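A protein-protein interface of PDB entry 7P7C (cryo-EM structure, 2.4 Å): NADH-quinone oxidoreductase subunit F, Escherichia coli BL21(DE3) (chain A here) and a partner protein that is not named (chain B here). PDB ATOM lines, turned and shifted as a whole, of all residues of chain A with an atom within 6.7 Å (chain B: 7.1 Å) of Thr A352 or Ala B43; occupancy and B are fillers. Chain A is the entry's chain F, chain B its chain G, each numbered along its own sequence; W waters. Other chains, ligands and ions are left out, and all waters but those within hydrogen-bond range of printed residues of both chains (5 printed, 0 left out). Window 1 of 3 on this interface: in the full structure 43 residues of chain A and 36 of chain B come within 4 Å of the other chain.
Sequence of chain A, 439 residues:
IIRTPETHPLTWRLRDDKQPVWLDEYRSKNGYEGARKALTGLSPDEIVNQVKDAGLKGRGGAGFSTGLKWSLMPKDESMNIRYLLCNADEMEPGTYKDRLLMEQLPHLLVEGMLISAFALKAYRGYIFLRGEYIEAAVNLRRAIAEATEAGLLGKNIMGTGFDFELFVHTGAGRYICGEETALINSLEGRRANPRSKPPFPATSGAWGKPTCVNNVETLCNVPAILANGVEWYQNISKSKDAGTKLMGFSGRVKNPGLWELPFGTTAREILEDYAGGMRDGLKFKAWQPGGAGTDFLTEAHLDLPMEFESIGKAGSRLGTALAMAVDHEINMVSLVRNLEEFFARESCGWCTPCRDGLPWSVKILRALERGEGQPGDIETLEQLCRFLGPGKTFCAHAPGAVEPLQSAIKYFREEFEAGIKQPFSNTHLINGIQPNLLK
The side-chain hydroxyl (OH) of Tyr B154 lies within hydrogen-bond range of the backbone carbonyl oxygen (O) of Gly A349 (2.7 Å). OG1 of Thr A352 lies within hydrogen-bond range of O of Cys B44 (2.9 Å). The backbone carbonyl oxygen of Ile B151 lies within hydrogen-bond range of the guanidinium group of Arg A355 (3.0 Å). The backbone carbonyl oxygen (O) of Thr A393 sits at hydrogen-bond distance from the guanidinium group (NH2) of Arg B45 (3.2 Å).
Of the 13 printed residues of chain A, 11 touch a printed residue of chain B. Printed residues of chain B that touch a printed residue of chain A: Val B41, Gly B42, Ala B43, Cys B44, Arg B45, Trp B93, Leu B94, Ile B151, Ala B152 and Tyr B154. Hydrophobic or aromatic side chains of chain B within 4 Å of the printed part of chain A: Val B41, Ala B43, Trp B93, Leu B94, Ala B152 and Tyr B154. Among the printed residues, 23 pairs touch across the chains.
Thr A352 touches three residues of chain B. Printed residues of chain A within 4 Å of Ala B43: Trp A350, Cys A351 and Thr A352. Of the printed residues of chain A, Gly B42 touches Trp A350 (3.8 Å) and Phe A394 (3.2 Å). Of the printed residues of chain B, Gly A357 touches Trp B93. Of the printed residues of chain B, Leu A388 touches Trp B93. Of the printed residues of chain A, Ile B151 touches Arg A355 (3.0 Å). The nearest printed residue of chain B that does not touch Thr A352 is Val B90 (4.1 Å).
Among the printed residues, pairs that only touch across the chains: Cys A351 with Ala B43 (3.2 Å), Phe A394 with Gly B42 (3.2 Å), Phe A394 with Val B41 (3.3 Å), Trp A350 with Tyr B154 (3.4 Å), Arg A355 with Ala B152 (3.5 Å), Pro A353 with Trp B93 (3.5 Å), Phe A394 with Arg B45 (3.6 Å), Asp A356 with Trp B93 (3.6 Å), Pro A353 with Arg B45 (3.6 Å), Thr A352 with Ala B43 (3.6 Å), Trp A350 with Ala B43 (3.6 Å), Trp A350 with Val B41 (3.6 Å), Thr A352 with Leu B94 (3.7 Å), Asp A356 with Leu B94 (3.7 Å), Leu A388 with Trp B93 (3.7 Å), Trp A350 with Gly B42 (3.8 Å), Arg A355 with Leu B94 (3.8 Å), Gly A357 with Trp B93 (3.9 Å) and Cys A351 with Arg B45 (3.96 Å).
Water W5 lies within hydrogen-bond range of the backbone carbonyl oxygen of Ile B151 (2.8 Å) and the side-chain hydroxyl of Thr A352 (3.4 Å). Water W1 lies within hydrogen-bond range of OD2 of Asp A356 (2.9 Å) and O of Ile B151 (3.4 Å). Water W3 lies within hydrogen-bond range of the backbone carbonyl oxygen of Trp B93 and the side-chain carboxylate of Asp A356.
NH1 of Arg A355 is in hydrogen-bond range of O of Trp A350, 3.3 Å away. The backbone NH (N) of Phe A394 sits close to the side-chain sulfur (SG) of Cys A351 (3.3 Å). OD2 of Asp A356 lies within salt-bridge range of NE of Arg A355, at 3.4 Å. O of Gly B42 sits at hydrogen-bond distance from NH1 of Arg B45. SD of Met B67 sits at hydrogen-bond distance from N of Gly B42, 3.6 Å away.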
ATOM      1  N   GLY A 349      25.187  31.688  16.044  1.00  0.00           N
ATOM      2  CA  GLY A 349      24.704  30.416  16.528  1.00  0.00           C
ATOM      3  C   GLY A 349      23.481  30.471  17.410  1.00  0.00           C
ATOM      4  O   GLY A 349      23.075  29.430  17.934  1.00  0.00           O
ATOM      5  N   TRP A 350      22.883  31.647  17.595  1.00  0.00           N
ATOM      6  CA  TRP A 350      21.742  31.769  18.494  1.00  0.00           C
ATOM      7  C   TRP A 350      20.498  31.108  17.916  1.00  0.00           C
ATOM      8  O   TRP A 350      19.824  30.333  18.602  1.00  0.00           O
ATOM      9  CB  TRP A 350      21.468  33.240  18.798  1.00  0.00           C
ATOM     10  CG  TRP A 350      20.281  33.497  19.668  1.00  0.00           C
ATOM     11  CD1 TRP A 350      19.124  34.118  19.306  1.00  0.00           C
ATOM     12  CD2 TRP A 350      20.141  33.161  21.050  1.00  0.00           C
ATOM     13  NE1 TRP A 350      18.268  34.185  20.373  1.00  0.00           N
ATOM     14  CE2 TRP A 350      18.868  33.604  21.458  1.00  0.00           C
ATOM     15  CE3 TRP A 350      20.964  32.527  21.982  1.00  0.00           C
ATOM     16  CZ2 TRP A 350      18.401  33.432  22.756  1.00  0.00           C
ATOM     17  CZ3 TRP A 350      20.497  32.356  23.269  1.00  0.00           C
ATOM     18  CH2 TRP A 350      19.229  32.806  23.645  1.00  0.00           C
ATOM     19  N   CYS A 351      20.175  31.390  16.659  1.00  0.00           N
ATOM     20  CA  CYS A 351      18.872  31.022  16.138  1.00  0.00           C
ATOM     21  C   CYS A 351      18.981  30.063  14.959  1.00  0.00           C
ATOM     22  O   CYS A 351      19.920  30.123  14.163  1.00  0.00           O
ATOM     23  CB  CYS A 351      18.048  32.271  15.780  1.00  0.00           C
ATOM     24  SG  CYS A 351      18.400  33.121  14.258  1.00  0.00           S
ATOM     25  N   THR A 352      17.986  29.175  14.879  1.00  0.00           N
ATOM     26  CA  THR A 352      18.027  28.022  13.978  1.00  0.00           C
ATOM     27  C   THR A 352      18.151  28.347  12.488  1.00  0.00           C
ATOM     28  O   THR A 352      18.984  27.706  11.828  1.00  0.00           O
ATOM     29  CB  THR A 352      16.802  27.138  14.238  1.00  0.00           C
ATOM     30  OG1 THR A 352      16.766  26.757  15.617  1.00  0.00           O
ATOM     31  CG2 THR A 352      16.834  25.891  13.377  1.00  0.00           C
ATOM     32  N   PRO A 353      17.371  29.271  11.886  1.00  0.00           N
ATOM     33  CA  PRO A 353      17.444  29.409  10.416  1.00  0.00           C
ATOM     34  C   PRO A 353      18.806  29.833   9.901  1.00  0.00           C
ATOM     35  O   PRO A 353      19.325  29.202   8.984  1.00  0.00           O
ATOM     36  CB  PRO A 353      16.366  30.457  10.115  1.00  0.00           C
ATOM     37  CG  PRO A 353      15.452  30.378  11.243  1.00  0.00           C
ATOM     38  CD  PRO A 353      16.345  30.190  12.408  1.00  0.00           C
ATOM     39  N   CYS A 354      19.432  30.830  10.522  1.00  0.00           N
ATOM     40  CA  CYS A 354      20.777  31.230  10.126  1.00  0.00           C
ATOM     41  C   CYS A 354      21.779  30.108  10.371  1.00  0.00           C
ATOM     42  O   CYS A 354      22.407  29.616   9.423  1.00  0.00           O
ATOM     43  CB  CYS A 354      21.146  32.499  10.889  1.00  0.00           C
ATOM     44  SG  CYS A 354      22.818  33.168  10.860  1.00  0.00           S
ATOM     45  N   ARG A 355      21.806  29.592  11.607  1.00  0.00           N
ATOM     46  CA  ARG A 355      22.824  28.641  12.050  1.00  0.00           C
ATOM     47  C   ARG A 355      22.781  27.335  11.264  1.00  0.00           C
ATOM     48  O   ARG A 355      23.828  26.767  10.937  1.00  0.00           O
ATOM     49  CB  ARG A 355      22.653  28.369  13.549  1.00  0.00           C
ATOM     50  CG  ARG A 355      23.278  27.070  14.043  1.00  0.00           C
ATOM     51  CD  ARG A 355      22.991  26.788  15.510  1.00  0.00           C
ATOM     52  NE  ARG A 355      21.762  26.025  15.667  1.00  0.00           N
ATOM     53  CZ  ARG A 355      20.651  26.498  16.215  1.00  0.00           C
ATOM     54  NH1 ARG A 355      20.601  27.712  16.733  1.00  0.00           N
ATOM     55  NH2 ARG A 355      19.568  25.731  16.247  1.00  0.00           N
ATOM     56  N   ASP A 356      21.587  26.842  10.945  1.00  0.00           N
ATOM     57  CA  ASP A 356      21.438  25.551  10.290  1.00  0.00           C
ATOM     58  C   ASP A 356      20.937  25.651   8.855  1.00  0.00           C
ATOM     59  O   ASP A 356      20.705  24.616   8.225  1.00  0.00           O
ATOM     60  CB  ASP A 356      20.504  24.652  11.101  1.00  0.00           C
ATOM     61  CG  ASP A 356      21.097  24.248  12.432  1.00  0.00           C
ATOM     62  OD1 ASP A 356      22.338  24.216  12.549  1.00  0.00           O
ATOM     63  OD2 ASP A 356      20.321  23.959  13.362  1.00  0.00           O
ATOM     64  N   GLY A 357      20.778  26.852   8.308  1.00  0.00           N
ATOM     65  CA  GLY A 357      20.344  26.959   6.938  1.00  0.00           C
ATOM     66  C   GLY A 357      21.392  27.595   6.061  1.00  0.00           C
ATOM     67  O   GLY A 357      21.459  27.282   4.871  1.00  0.00           O
ATOM     68  N   LEU A 358      22.207  28.496   6.616  1.00  0.00           N
ATOM     69  CA  LEU A 358      23.349  28.987   5.853  1.00  0.00           C
ATOM     70  C   LEU A 358      24.363  27.898   5.487  1.00  0.00           C
ATOM     71  O   LEU A 358      24.818  27.905   4.330  1.00  0.00           O
ATOM     72  CB  LEU A 358      24.004  30.155   6.604  1.00  0.00           C
ATOM     73  CG  LEU A 358      23.188  31.448   6.602  1.00  0.00           C
ATOM     74  CD1 LEU A 358      23.925  32.555   7.326  1.00  0.00           C
ATOM     75  CD2 LEU A 358      22.857  31.861   5.181  1.00  0.00           C
ATOM     76  N   LEU A 388      14.713  32.841   5.418  1.00  0.00           N
ATOM     77  CA  LEU A 388      15.707  33.508   6.247  1.00  0.00           C
ATOM     78  C   LEU A 388      15.555  35.022   6.200  1.00  0.00           C
ATOM     79  O   LEU A 388      16.490  35.747   6.546  1.00  0.00           O
ATOM     80  CB  LEU A 388      17.119  33.101   5.830  1.00  0.00           C
ATOM     81  CG  LEU A 388      17.793  31.974   6.615  1.00  0.00           C
ATOM     82  CD1 LEU A 388      17.102  30.646   6.376  1.00  0.00           C
ATOM     83  CD2 LEU A 388      19.260  31.879   6.246  1.00  0.00           C
ATOM     84  N   THR A 393      14.411  35.262  11.453  1.00  0.00           N
ATOM     85  CA  THR A 393      15.594  35.068  12.273  1.00  0.00           C
ATOM     86  C   THR A 393      15.623  36.091  13.402  1.00  0.00           C
ATOM     87  O   THR A 393      14.875  37.068  13.413  1.00  0.00           O
ATOM     88  CB  THR A 393      16.863  35.166  11.425  1.00  0.00           C
ATOM     89  OG1 THR A 393      16.946  36.466  10.834  1.00  0.00           O
ATOM     90  CG2 THR A 393      16.841  34.121  10.331  1.00  0.00           C
ATOM     91  N   PHE A 394      16.511  35.848  14.363  1.00  0.00           N
ATOM     92  CA  PHE A 394      16.552  36.677  15.561  1.00  0.00           C
ATOM     93  C   PHE A 394      17.168  38.043  15.292  1.00  0.00           C
ATOM     94  O   PHE A 394      16.813  39.019  15.960  1.00  0.00           O
ATOM     95  CB  PHE A 394      17.313  35.943  16.662  1.00  0.00           C
ATOM     96  CG  PHE A 394      17.225  36.597  18.003  1.00  0.00           C
ATOM     97  CD1 PHE A 394      16.104  36.430  18.797  1.00  0.00           C
ATOM     98  CD2 PHE A 394      18.272  37.362  18.484  1.00  0.00           C
ATOM     99  CE1 PHE A 394      16.026  37.024  20.035  1.00  0.00           C
ATOM    100  CE2 PHE A 394      18.198  37.955  19.721  1.00  0.00           C
ATOM    101  CZ  PHE A 394      17.075  37.783  20.499  1.00  0.00           C
ATOM    102  N   PHE B  32      10.693  24.737  21.057  1.00  0.00           N
ATOM    103  CA  PHE B  32      11.832  24.130  21.732  1.00  0.00           C
ATOM    104  C   PHE B  32      12.416  24.998  22.833  1.00  0.00           C
ATOM    105  O   PHE B  32      12.517  24.548  23.976  1.00  0.00           O
ATOM    106  CB  PHE B  32      12.918  23.773  20.713  1.00  0.00           C
ATOM    107  CG  PHE B  32      12.533  22.653  19.806  1.00  0.00           C
ATOM    108  CD1 PHE B  32      12.402  21.368  20.297  1.00  0.00           C
ATOM    109  CD2 PHE B  32      12.282  22.884  18.467  1.00  0.00           C
ATOM    110  CE1 PHE B  32      12.046  20.335  19.466  1.00  0.00           C
ATOM    111  CE2 PHE B  32      11.922  21.850  17.636  1.00  0.00           C
ATOM    112  CZ  PHE B  32      11.806  20.579  18.134  1.00  0.00           C
ATOM    113  N   CYS B  33      12.783  26.241  22.533  1.00  0.00           N
ATOM    114  CA  CYS B  33      13.616  27.004  23.453  1.00  0.00           C
ATOM    115  C   CYS B  33      12.839  27.628  24.605  1.00  0.00           C
ATOM    116  O   CYS B  33      13.458  28.035  25.590  1.00  0.00           O
ATOM    117  CB  CYS B  33      14.385  28.088  22.689  1.00  0.00           C
ATOM    118  SG  CYS B  33      13.438  29.533  22.224  1.00  0.00           S
ATOM    119  N   TRP B  34      11.516  27.701  24.521  1.00  0.00           N
ATOM    120  CA  TRP B  34      10.708  28.234  25.608  1.00  0.00           C
ATOM    121  C   TRP B  34      10.431  27.158  26.646  1.00  0.00           C
ATOM    122  O   TRP B  34      10.203  25.994  26.310  1.00  0.00           O
ATOM    123  CB  TRP B  34       9.389  28.793  25.078  1.00  0.00           C
ATOM    124  CG  TRP B  34       8.422  29.210  26.141  1.00  0.00           C
ATOM    125  CD1 TRP B  34       8.393  30.399  26.799  1.00  0.00           C
ATOM    126  CD2 TRP B  34       7.339  28.437  26.665  1.00  0.00           C
ATOM    127  NE1 TRP B  34       7.362  30.419  27.700  1.00  0.00           N
ATOM    128  CE2 TRP B  34       6.698  29.224  27.637  1.00  0.00           C
ATOM    129  CE3 TRP B  34       6.850  27.154  26.408  1.00  0.00           C
ATOM    130  CZ2 TRP B  34       5.594  28.773  28.352  1.00  0.00           C
ATOM    131  CZ3 TRP B  34       5.756  26.709  27.116  1.00  0.00           C
ATOM    132  CH2 TRP B  34       5.138  27.517  28.075  1.00  0.00           C
ATOM    133  N   SER B  40      10.923  33.371  27.936  1.00  0.00           N
ATOM    134  CA  SER B  40      11.079  33.334  26.491  1.00  0.00           C
ATOM    135  C   SER B  40      12.360  34.039  26.073  1.00  0.00           C
ATOM    136  O   SER B  40      12.707  35.091  26.616  1.00  0.00           O
ATOM    137  CB  SER B  40       9.891  33.993  25.800  1.00  0.00           C
ATOM    138  OG  SER B  40       8.664  33.488  26.283  1.00  0.00           O
ATOM    139  N   VAL B  41      13.062  33.451  25.106  1.00  0.00           N
ATOM    140  CA  VAL B  41      14.240  34.087  24.521  1.00  0.00           C
ATOM    141  C   VAL B  41      14.198  34.154  23.005  1.00  0.00           C
ATOM    142  O   VAL B  41      14.969  34.925  22.410  1.00  0.00           O
ATOM    143  CB  VAL B  41      15.531  33.381  24.985  1.00  0.00           C
ATOM    144  CG1 VAL B  41      15.839  33.752  26.416  1.00  0.00           C
ATOM    145  CG2 VAL B  41      15.413  31.874  24.815  1.00  0.00           C
ATOM    146  N   GLY B  42      13.338  33.397  22.333  1.00  0.00           N
ATOM    147  CA  GLY B  42      13.242  33.453  20.885  1.00  0.00           C
ATOM    148  C   GLY B  42      14.429  32.905  20.124  1.00  0.00           C
ATOM    149  O   GLY B  42      14.814  33.472  19.096  1.00  0.00           O
ATOM    150  N   ALA B  43      15.015  31.806  20.594  1.00  0.00           N
ATOM    151  CA  ALA B  43      16.178  31.227  19.932  1.00  0.00           C
ATOM    152  C   ALA B  43      15.780  30.263  18.815  1.00  0.00           C
ATOM    153  O   ALA B  43      16.148  30.468  17.659  1.00  0.00           O
ATOM    154  CB  ALA B  43      17.070  30.519  20.956  1.00  0.00           C
ATOM    155  N   CYS B  44      15.011  29.225  19.139  1.00  0.00           N
ATOM    156  CA  CYS B  44      14.829  28.111  18.214  1.00  0.00           C
ATOM    157  C   CYS B  44      13.981  28.459  16.993  1.00  0.00           C
ATOM    158  O   CYS B  44      14.061  27.746  15.990  1.00  0.00           O
ATOM    159  CB  CYS B  44      14.210  26.928  18.950  1.00  0.00           C
ATOM    160  SG  CYS B  44      12.497  27.156  19.385  1.00  0.00           S
ATOM    161  N   ARG B  45      13.172  29.520  17.063  1.00  0.00           N
ATOM    162  CA  ARG B  45      12.274  29.985  15.995  1.00  0.00           C
ATOM    163  C   ARG B  45      11.245  28.933  15.583  1.00  0.00           C
ATOM    164  O   ARG B  45      10.691  29.005  14.487  1.00  0.00           O
ATOM    165  CB  ARG B  45      13.045  30.483  14.764  1.00  0.00           C
ATOM    166  CG  ARG B  45      14.267  31.338  15.072  1.00  0.00           C
ATOM    167  CD  ARG B  45      13.952  32.524  15.952  1.00  0.00           C
ATOM    168  NE  ARG B  45      13.306  33.599  15.216  1.00  0.00           N
ATOM    169  CZ  ARG B  45      13.044  34.793  15.727  1.00  0.00           C
ATOM    170  NH1 ARG B  45      13.361  35.094  16.972  1.00  0.00           N
ATOM    171  NH2 ARG B  45      12.443  35.703  14.969  1.00  0.00           N
ATOM    172  N   GLN B  46      10.964  27.963  16.453  1.00  0.00           N
ATOM    173  CA  GLN B  46      10.028  26.897  16.118  1.00  0.00           C
ATOM    174  C   GLN B  46       8.575  27.329  16.278  1.00  0.00           C
ATOM    175  O   GLN B  46       7.703  26.815  15.576  1.00  0.00           O
ATOM    176  CB  GLN B  46      10.315  25.668  16.983  1.00  0.00           C
ATOM    177  CG  GLN B  46       9.477  24.442  16.683  1.00  0.00           C
ATOM    178  CD  GLN B  46       9.725  23.903  15.297  1.00  0.00           C
ATOM    179  OE1 GLN B  46      10.698  23.196  15.064  1.00  0.00           O
ATOM    180  NE2 GLN B  46       8.847  24.237  14.367  1.00  0.00           N
ATOM    181  N   MET B  64       7.320  35.076  16.346  1.00  0.00           N
ATOM    182  CA  MET B  64       7.498  34.039  17.352  1.00  0.00           C
ATOM    183  C   MET B  64       6.439  34.229  18.427  1.00  0.00           C
ATOM    184  O   MET B  64       6.363  35.296  19.043  1.00  0.00           O
ATOM    185  CB  MET B  64       8.900  34.092  17.951  1.00  0.00           C
ATOM    186  CG  MET B  64       9.989  33.659  16.993  1.00  0.00           C
ATOM    187  SD  MET B  64       9.481  32.315  15.908  1.00  0.00           S
ATOM    188  CE  MET B  64       9.816  33.032  14.307  1.00  0.00           C
ATOM    189  N   CYS B  66       6.225  32.865  21.305  1.00  0.00           N
ATOM    190  CA  CYS B  66       6.775  32.973  22.651  1.00  0.00           C
ATOM    191  C   CYS B  66       7.268  34.383  22.947  1.00  0.00           C
ATOM    192  O   CYS B  66       7.296  34.793  24.108  1.00  0.00           O
ATOM    193  CB  CYS B  66       7.896  31.952  22.848  1.00  0.00           C
ATOM    194  SG  CYS B  66       9.455  32.340  22.043  1.00  0.00           S
ATOM    195  N   MET B  67       7.636  35.144  21.922  1.00  0.00           N
ATOM    196  CA  MET B  67       8.140  36.497  22.104  1.00  0.00           C
ATOM    197  C   MET B  67       7.093  37.567  21.832  1.00  0.00           C
ATOM    198  O   MET B  67       7.428  38.753  21.839  1.00  0.00           O
ATOM    199  CB  MET B  67       9.353  36.731  21.201  1.00  0.00           C
ATOM    200  CG  MET B  67      10.538  35.852  21.519  1.00  0.00           C
ATOM    201  SD  MET B  67      11.190  36.114  23.174  1.00  0.00           S
ATOM    202  CE  MET B  67      12.106  37.629  22.946  1.00  0.00           C
ATOM    203  N   SER B  89      10.159  23.705   8.150  1.00  0.00           N
ATOM    204  CA  SER B  89      11.522  24.013   7.725  1.00  0.00           C
ATOM    205  C   SER B  89      12.475  24.110   8.909  1.00  0.00           C
ATOM    206  O   SER B  89      13.643  23.733   8.797  1.00  0.00           O
ATOM    207  CB  SER B  89      11.543  25.311   6.922  1.00  0.00           C
ATOM    208  OG  SER B  89      11.041  25.101   5.620  1.00  0.00           O
ATOM    209  N   VAL B  90      12.006  24.642  10.038  1.00  0.00           N
ATOM    210  CA  VAL B  90      12.837  24.696  11.239  1.00  0.00           C
ATOM    211  C   VAL B  90      13.143  23.289  11.737  1.00  0.00           C
ATOM    212  O   VAL B  90      14.287  22.976  12.099  1.00  0.00           O
ATOM    213  CB  VAL B  90      12.155  25.557  12.321  1.00  0.00           C
ATOM    214  CG1 VAL B  90      12.827  25.375  13.677  1.00  0.00           C
ATOM    215  CG2 VAL B  90      12.186  27.015  11.921  1.00  0.00           C
ATOM    216  N   VAL B  91      12.132  22.411  11.728  1.00  0.00           N
ATOM    217  CA  VAL B  91      12.360  21.008  12.071  1.00  0.00           C
ATOM    218  C   VAL B  91      13.362  20.376  11.108  1.00  0.00           C
ATOM    219  O   VAL B  91      14.288  19.674  11.529  1.00  0.00           O
ATOM    220  CB  VAL B  91      11.020  20.244  12.100  1.00  0.00           C
ATOM    221  CG1 VAL B  91      11.210  18.772  11.778  1.00  0.00           C
ATOM    222  CG2 VAL B  91      10.370  20.389  13.452  1.00  0.00           C
ATOM    223  N   GLU B  92      13.225  20.663   9.810  1.00  0.00           N
ATOM    224  CA  GLU B  92      14.131  20.115   8.805  1.00  0.00           C
ATOM    225  C   GLU B  92      15.564  20.599   9.006  1.00  0.00           C
ATOM    226  O   GLU B  92      16.512  19.825   8.845  1.00  0.00           O
ATOM    227  CB  GLU B  92      13.638  20.482   7.407  1.00  0.00           C
ATOM    228  CG  GLU B  92      14.489  19.915   6.293  1.00  0.00           C
ATOM    229  CD  GLU B  92      13.917  20.184   4.922  1.00  0.00           C
ATOM    230  OE1 GLU B  92      13.053  21.072   4.794  1.00  0.00           O
ATOM    231  OE2 GLU B  92      14.331  19.501   3.968  1.00  0.00           O
ATOM    232  N   TRP B  93      15.737  21.878   9.347  1.00  0.00           N
ATOM    233  CA  TRP B  93      17.068  22.413   9.616  1.00  0.00           C
ATOM    234  C   TRP B  93      17.686  21.762  10.843  1.00  0.00           C
ATOM    235  O   TRP B  93      18.889  21.486  10.864  1.00  0.00           O
ATOM    236  CB  TRP B  93      17.006  23.927   9.806  1.00  0.00           C
ATOM    237  CG  TRP B  93      16.769  24.679   8.550  1.00  0.00           C
ATOM    238  CD1 TRP B  93      17.265  24.390   7.319  1.00  0.00           C
ATOM    239  CD2 TRP B  93      15.969  25.853   8.397  1.00  0.00           C
ATOM    240  NE1 TRP B  93      16.825  25.310   6.405  1.00  0.00           N
ATOM    241  CE2 TRP B  93      16.025  26.220   7.042  1.00  0.00           C
ATOM    242  CE3 TRP B  93      15.208  26.629   9.274  1.00  0.00           C
ATOM    243  CZ2 TRP B  93      15.352  27.330   6.542  1.00  0.00           C
ATOM    244  CZ3 TRP B  93      14.538  27.726   8.777  1.00  0.00           C
ATOM    245  CH2 TRP B  93      14.616  28.069   7.425  1.00  0.00           C
ATOM    246  N   LEU B  94      16.879  21.521  11.879  1.00  0.00           N
ATOM    247  CA  LEU B  94      17.383  20.792  13.038  1.00  0.00           C
ATOM    248  C   LEU B  94      17.731  19.351  12.690  1.00  0.00           C
ATOM    249  O   LEU B  94      18.619  18.762  13.313  1.00  0.00           O
ATOM    250  CB  LEU B  94      16.360  20.826  14.170  1.00  0.00           C
ATOM    251  CG  LEU B  94      16.097  22.199  14.780  1.00  0.00           C
ATOM    252  CD1 LEU B  94      15.054  22.088  15.869  1.00  0.00           C
ATOM    253  CD2 LEU B  94      17.382  22.799  15.316  1.00  0.00           C
ATOM    254  N   ILE B 151      20.201  20.351  19.529  1.00  0.00           N
ATOM    255  CA  ILE B 151      19.552  21.225  18.567  1.00  0.00           C
ATOM    256  C   ILE B 151      19.826  22.689  18.870  1.00  0.00           C
ATOM    257  O   ILE B 151      19.225  23.566  18.243  1.00  0.00           O
ATOM    258  CB  ILE B 151      18.044  20.951  18.495  1.00  0.00           C
ATOM    259  CG1 ILE B 151      17.398  21.184  19.859  1.00  0.00           C
ATOM    260  CG2 ILE B 151      17.788  19.538  18.007  1.00  0.00           C
ATOM    261  CD1 ILE B 151      15.924  20.980  19.874  1.00  0.00           C
ATOM    262  N   ALA B 152      20.724  22.967  19.826  1.00  0.00           N
ATOM    263  CA  ALA B 152      21.153  24.320  20.202  1.00  0.00           C
ATOM    264  C   ALA B 152      19.969  25.201  20.594  1.00  0.00           C
ATOM    265  O   ALA B 152      19.801  26.314  20.099  1.00  0.00           O
ATOM    266  CB  ALA B 152      21.983  24.971  19.094  1.00  0.00           C
ATOM    267  N   CYS B 153      19.133  24.680  21.481  1.00  0.00           N
ATOM    268  CA  CYS B 153      17.960  25.405  21.937  1.00  0.00           C
ATOM    269  C   CYS B 153      18.219  26.235  23.188  1.00  0.00           C
ATOM    270  O   CYS B 153      17.322  26.963  23.619  1.00  0.00           O
ATOM    271  CB  CYS B 153      16.816  24.426  22.191  1.00  0.00           C
ATOM    272  SG  CYS B 153      16.911  23.564  23.754  1.00  0.00           S
ATOM    273  N   TYR B 154      19.404  26.116  23.784  1.00  0.00           N
ATOM    274  CA  TYR B 154      19.900  26.910  24.909  1.00  0.00           C
ATOM    275  C   TYR B 154      19.111  26.707  26.198  1.00  0.00           C
ATOM    276  O   TYR B 154      19.307  27.462  27.146  1.00  0.00           O
ATOM    277  CB  TYR B 154      19.957  28.410  24.573  1.00  0.00           C
ATOM    278  CG  TYR B 154      20.966  28.762  23.510  1.00  0.00           C
ATOM    279  CD1 TYR B 154      20.668  28.602  22.167  1.00  0.00           C
ATOM    280  CD2 TYR B 154      22.220  29.249  23.849  1.00  0.00           C
ATOM    281  CE1 TYR B 154      21.585  28.913  21.192  1.00  0.00           C
ATOM    282  CE2 TYR B 154      23.143  29.565  22.881  1.00  0.00           C
ATOM    283  CZ  TYR B 154      22.819  29.394  21.554  1.00  0.00           C
ATOM    284  OH  TYR B 154      23.729  29.706  20.577  1.00  0.00           O
ATOM    285  N   ARG B 158      20.317  28.101  30.111  1.00  0.00           N
ATOM    286  CA  ARG B 158      19.392  29.043  30.730  1.00  0.00           C
ATOM    287  C   ARG B 158      18.890  28.522  32.070  1.00  0.00           C
ATOM    288  O   ARG B 158      18.989  29.223  33.079  1.00  0.00           O
ATOM    289  CB  ARG B 158      18.236  29.345  29.780  1.00  0.00           C
ATOM    290  CG  ARG B 158      18.666  30.200  28.605  1.00  0.00           C
ATOM    291  CD  ARG B 158      17.538  31.016  28.044  1.00  0.00           C
ATOM    292  NE  ARG B 158      16.357  30.222  27.737  1.00  0.00           N
ATOM    293  CZ  ARG B 158      15.173  30.398  28.302  1.00  0.00           C
ATOM    294  NH1 ARG B 158      14.984  31.311  29.239  1.00  0.00           N
ATOM    295  NH2 ARG B 158      14.151  29.641  27.917  1.00  0.00           N
HETATM  296  O   HOH W   1      21.212  22.425  15.695  1.00  0.00           O
HETATM  297  O   HOH W   2      12.836  38.372  15.608  1.00  0.00           O
HETATM  298  O   HOH W   3      21.351  20.951  12.710  1.00  0.00           O
HETATM  299  O   HOH W   4      18.416  27.811  18.446  1.00  0.00           O
HETATM  300  O   HOH W   5      16.862  25.002  18.502  1.00  0.00           O
